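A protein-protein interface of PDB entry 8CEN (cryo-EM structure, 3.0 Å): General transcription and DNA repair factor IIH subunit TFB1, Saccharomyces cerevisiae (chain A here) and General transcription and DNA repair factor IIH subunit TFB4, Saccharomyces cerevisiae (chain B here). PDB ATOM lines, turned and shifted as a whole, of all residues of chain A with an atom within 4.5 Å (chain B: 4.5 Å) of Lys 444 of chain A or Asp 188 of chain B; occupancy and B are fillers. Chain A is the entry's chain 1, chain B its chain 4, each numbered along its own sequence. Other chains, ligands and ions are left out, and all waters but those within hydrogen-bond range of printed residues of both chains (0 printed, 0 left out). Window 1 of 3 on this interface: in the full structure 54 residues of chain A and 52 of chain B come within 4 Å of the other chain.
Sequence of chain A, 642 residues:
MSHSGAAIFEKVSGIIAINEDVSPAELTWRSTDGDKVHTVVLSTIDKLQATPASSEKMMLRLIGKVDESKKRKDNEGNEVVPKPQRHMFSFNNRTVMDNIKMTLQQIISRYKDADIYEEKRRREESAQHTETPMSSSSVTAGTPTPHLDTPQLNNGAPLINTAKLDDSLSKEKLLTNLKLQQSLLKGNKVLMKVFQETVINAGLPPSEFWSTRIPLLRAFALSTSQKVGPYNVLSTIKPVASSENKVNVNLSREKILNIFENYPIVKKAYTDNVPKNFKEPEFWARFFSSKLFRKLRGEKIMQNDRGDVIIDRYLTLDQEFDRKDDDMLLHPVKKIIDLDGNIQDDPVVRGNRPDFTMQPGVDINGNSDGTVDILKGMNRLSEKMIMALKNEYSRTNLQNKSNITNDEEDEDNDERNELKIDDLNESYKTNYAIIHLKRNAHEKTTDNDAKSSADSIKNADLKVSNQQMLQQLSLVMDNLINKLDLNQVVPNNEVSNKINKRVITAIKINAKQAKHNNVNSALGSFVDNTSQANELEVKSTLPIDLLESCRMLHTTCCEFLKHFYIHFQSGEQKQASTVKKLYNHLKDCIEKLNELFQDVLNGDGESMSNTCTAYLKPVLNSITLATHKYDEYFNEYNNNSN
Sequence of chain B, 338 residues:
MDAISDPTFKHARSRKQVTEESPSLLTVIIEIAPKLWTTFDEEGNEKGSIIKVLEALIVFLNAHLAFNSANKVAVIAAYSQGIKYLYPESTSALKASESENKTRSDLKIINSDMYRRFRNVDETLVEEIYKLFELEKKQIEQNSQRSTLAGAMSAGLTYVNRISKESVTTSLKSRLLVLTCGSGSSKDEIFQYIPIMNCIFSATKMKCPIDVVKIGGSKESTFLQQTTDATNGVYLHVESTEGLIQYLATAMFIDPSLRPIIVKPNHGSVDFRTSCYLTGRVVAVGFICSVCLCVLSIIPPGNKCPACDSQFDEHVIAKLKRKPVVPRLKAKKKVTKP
Among the printed residues, merely in contact across the chains: His 442 of chain A with Ile 190 of chain B (3.7 Å), Glu 443 of chain A with Asp 188 of chain B (3.6 Å), Glu 443 of chain A with Gly 280 of chain B (3.4 Å) and Lys 444 of chain A with Gly 280 of chain B (3.3 Å).
Lys 444 of chain A touches just these residues of chain B: Asp 188 (3.5 Å) and Gly 280 (3.3 Å). Of chain A, only Glu 443 (3.6 Å) and Lys 444 (3.5 Å) come within 4 Å of Asp 188 of chain B. Of the printed residues of chain B, Glu 443 of chain A touches Asp 188 (3.6 Å) and Gly 280 (3.4 Å). Of the printed residues of chain A, Gly 280 of chain B touches Glu 443 (3.4 Å), Lys 444 (3.3 Å) and Thr 445 (3.4 Å). Printed residues of chain B within 4 Å of His 442 of chain A: Ile 190 (3.7 Å). Phe 223 of chain B touches none of the printed residues of chain A. The nearest printed residue of chain A that does not touch Asp 188 of chain B is His 442 of chain A (7.3 Å).
The backbone carbonyl oxygen (O) of Gly 280 of chain B is in hydrogen-bond range of the backbone NH (N) of Thr 445 of chain A (3.4 Å). OD2 of Asp 188 of chain B is in salt-bridge range of NZ of Lys 444 of chain A, 3.6 Å away.
Of the 9 printed residues of chain B, 3 touch a printed residue of chain A. Printed residues of chain B that touch a printed residue of chain A: Asp 188, Ile 190 and Gly 280. Hydrophobic or aromatic side chains of chain B that line the printed part of chain A: Ile 190.
O of Gly 280 of chain B sits at hydrogen-bond distance from OG of Ser 275 of chain B.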
ATOM      1  N   HIS A 442     -32.411  14.788   7.340  1.00  0.00           N
ATOM      2  CA  HIS A 442     -31.127  14.105   7.393  1.00  0.00           C
ATOM      3  C   HIS A 442     -30.124  14.786   6.468  1.00  0.00           C
ATOM      4  O   HIS A 442     -30.481  15.328   5.419  1.00  0.00           O
ATOM      5  CB  HIS A 442     -31.285  12.635   7.006  1.00  0.00           C
ATOM      6  CG  HIS A 442     -30.068  11.806   7.274  1.00  0.00           C
ATOM      7  ND1 HIS A 442     -29.058  11.647   6.349  1.00  0.00           N
ATOM      8  CD2 HIS A 442     -29.697  11.092   8.362  1.00  0.00           C
ATOM      9  CE1 HIS A 442     -28.118  10.870   6.857  1.00  0.00           C
ATOM     10  NE2 HIS A 442     -28.481  10.520   8.077  1.00  0.00           N
ATOM     11  N   GLU A 443     -28.858  14.762   6.876  1.00  0.00           N
ATOM     12  CA  GLU A 443     -27.800  15.367   6.084  1.00  0.00           C
ATOM     13  C   GLU A 443     -27.553  14.560   4.812  1.00  0.00           C
ATOM     14  O   GLU A 443     -27.882  13.374   4.722  1.00  0.00           O
ATOM     15  CB  GLU A 443     -26.511  15.473   6.901  1.00  0.00           C
ATOM     16  CG  GLU A 443     -26.639  16.328   8.153  1.00  0.00           C
ATOM     17  CD  GLU A 443     -26.837  17.799   7.842  1.00  0.00           C
ATOM     18  OE1 GLU A 443     -26.300  18.272   6.817  1.00  0.00           O
ATOM     19  OE2 GLU A 443     -27.532  18.483   8.623  1.00  0.00           O
ATOM     20  N   LYS A 444     -26.974  15.229   3.817  1.00  0.00           N
ATOM     21  CA  LYS A 444     -26.727  14.597   2.527  1.00  0.00           C
ATOM     22  C   LYS A 444     -25.638  13.538   2.651  1.00  0.00           C
ATOM     23  O   LYS A 444     -24.580  13.784   3.238  1.00  0.00           O
ATOM     24  CB  LYS A 444     -26.331  15.645   1.489  1.00  0.00           C
ATOM     25  CG  LYS A 444     -26.378  15.144   0.054  1.00  0.00           C
ATOM     26  CD  LYS A 444     -25.859  16.190  -0.919  1.00  0.00           C
ATOM     27  CE  LYS A 444     -24.351  16.346  -0.809  1.00  0.00           C
ATOM     28  NZ  LYS A 444     -23.831  17.375  -1.752  1.00  0.00           N
ATOM     29  N   THR A 445     -25.903  12.357   2.097  1.00  0.00           N
ATOM     30  CA  THR A 445     -24.976  11.237   2.145  1.00  0.00           C
ATOM     31  C   THR A 445     -24.843  10.625   0.759  1.00  0.00           C
ATOM     32  O   THR A 445     -25.758  10.707  -0.065  1.00  0.00           O
ATOM     33  CB  THR A 445     -25.435  10.159   3.142  1.00  0.00           C
ATOM     34  OG1 THR A 445     -26.836   9.910   2.971  1.00  0.00           O
ATOM     35  CG2 THR A 445     -25.171  10.602   4.575  1.00  0.00           C
ATOM     36  N   SER B 186     -16.861  22.366   5.290  1.00  0.00           N
ATOM     37  CA  SER B 186     -18.307  22.395   5.446  1.00  0.00           C
ATOM     38  C   SER B 186     -18.958  21.623   4.307  1.00  0.00           C
ATOM     39  O   SER B 186     -18.692  21.895   3.131  1.00  0.00           O
ATOM     40  CB  SER B 186     -18.821  23.835   5.473  1.00  0.00           C
ATOM     41  OG  SER B 186     -18.601  24.479   4.230  1.00  0.00           O
ATOM     42  N   LYS B 187     -19.807  20.661   4.658  1.00  0.00           N
ATOM     43  CA  LYS B 187     -20.505  19.853   3.668  1.00  0.00           C
ATOM     44  C   LYS B 187     -21.727  20.618   3.157  1.00  0.00           C
ATOM     45  O   LYS B 187     -21.915  21.804   3.442  1.00  0.00           O
ATOM     46  CB  LYS B 187     -20.883  18.500   4.264  1.00  0.00           C
ATOM     47  CG  LYS B 187     -19.711  17.547   4.444  1.00  0.00           C
ATOM     48  CD  LYS B 187     -18.988  17.296   3.129  1.00  0.00           C
ATOM     49  CE  LYS B 187     -17.798  16.370   3.324  1.00  0.00           C
ATOM     50  NZ  LYS B 187     -17.081  16.103   2.046  1.00  0.00           N
ATOM     51  N   ASP B 188     -22.571  19.942   2.381  1.00  0.00           N
ATOM     52  CA  ASP B 188     -23.797  20.558   1.892  1.00  0.00           C
ATOM     53  C   ASP B 188     -24.774  20.763   3.043  1.00  0.00           C
ATOM     54  O   ASP B 188     -24.988  19.861   3.858  1.00  0.00           O
ATOM     55  CB  ASP B 188     -24.430  19.695   0.803  1.00  0.00           C
ATOM     56  CG  ASP B 188     -25.402  20.473  -0.062  1.00  0.00           C
ATOM     57  OD1 ASP B 188     -25.353  21.721  -0.036  1.00  0.00           O
ATOM     58  OD2 ASP B 188     -26.212  19.837  -0.769  1.00  0.00           O
ATOM     59  N   GLU B 189     -25.367  21.951   3.107  1.00  0.00           N
ATOM     60  CA  GLU B 189     -26.230  22.336   4.214  1.00  0.00           C
ATOM     61  C   GLU B 189     -27.684  22.265   3.763  1.00  0.00           C
ATOM     62  O   GLU B 189     -28.080  22.957   2.819  1.00  0.00           O
ATOM     63  CB  GLU B 189     -25.879  23.738   4.707  1.00  0.00           C
ATOM     64  CG  GLU B 189     -24.409  23.916   5.075  1.00  0.00           C
ATOM     65  CD  GLU B 189     -23.975  23.054   6.249  1.00  0.00           C
ATOM     66  OE1 GLU B 189     -24.807  22.771   7.136  1.00  0.00           O
ATOM     67  OE2 GLU B 189     -22.790  22.656   6.282  1.00  0.00           O
ATOM     68  N   ILE B 190     -28.472  21.429   4.443  1.00  0.00           N
ATOM     69  CA  ILE B 190     -29.856  21.196   4.040  1.00  0.00           C
ATOM     70  C   ILE B 190     -30.714  22.427   4.313  1.00  0.00           C
ATOM     71  O   ILE B 190     -31.595  22.775   3.516  1.00  0.00           O
ATOM     72  CB  ILE B 190     -30.406  19.942   4.748  1.00  0.00           C
ATOM     73  CG1 ILE B 190     -29.551  18.715   4.418  1.00  0.00           C
ATOM     74  CG2 ILE B 190     -31.844  19.674   4.341  1.00  0.00           C
ATOM     75  CD1 ILE B 190     -29.276  18.522   2.937  1.00  0.00           C
ATOM     76  N   THR B 222     -24.200  22.105  -5.378  1.00  0.00           N
ATOM     77  CA  THR B 222     -25.406  21.876  -6.170  1.00  0.00           C
ATOM     78  C   THR B 222     -26.380  23.045  -6.088  1.00  0.00           C
ATOM     79  O   THR B 222     -26.986  23.420  -7.097  1.00  0.00           O
ATOM     80  CB  THR B 222     -26.088  20.585  -5.720  1.00  0.00           C
ATOM     81  OG1 THR B 222     -26.475  20.703  -4.344  1.00  0.00           O
ATOM     82  CG2 THR B 222     -25.145  19.403  -5.876  1.00  0.00           C
ATOM     83  N   PHE B 223     -26.535  23.636  -4.902  1.00  0.00           N
ATOM     84  CA  PHE B 223     -27.531  24.691  -4.721  1.00  0.00           C
ATOM     85  C   PHE B 223     -27.141  25.954  -5.480  1.00  0.00           C
ATOM     86  O   PHE B 223     -27.965  26.548  -6.184  1.00  0.00           O
ATOM     87  CB  PHE B 223     -27.717  24.988  -3.231  1.00  0.00           C
ATOM     88  CG  PHE B 223     -28.228  23.815  -2.429  1.00  0.00           C
ATOM     89  CD1 PHE B 223     -28.910  22.770  -3.038  1.00  0.00           C
ATOM     90  CD2 PHE B 223     -28.015  23.758  -1.062  1.00  0.00           C
ATOM     91  CE1 PHE B 223     -29.368  21.696  -2.299  1.00  0.00           C
ATOM     92  CE2 PHE B 223     -28.474  22.687  -0.319  1.00  0.00           C
ATOM     93  CZ  PHE B 223     -29.152  21.656  -0.938  1.00  0.00           C
ATOM     94  N   SER B 275     -32.488  16.275  -2.315  1.00  0.00           N
ATOM     95  CA  SER B 275     -32.051  15.303  -1.324  1.00  0.00           C
ATOM     96  C   SER B 275     -33.254  14.704  -0.611  1.00  0.00           C
ATOM     97  O   SER B 275     -34.240  15.398  -0.343  1.00  0.00           O
ATOM     98  CB  SER B 275     -31.109  15.949  -0.306  1.00  0.00           C
ATOM     99  OG  SER B 275     -30.706  15.014   0.679  1.00  0.00           O
ATOM    100  N   GLY B 280     -31.096  11.202   2.792  1.00  0.00           N
ATOM    101  CA  GLY B 280     -30.141  12.223   2.426  1.00  0.00           C
ATOM    102  C   GLY B 280     -29.516  12.067   1.056  1.00  0.00           C
ATOM    103  O   GLY B 280     -28.871  13.009   0.581  1.00  0.00           O
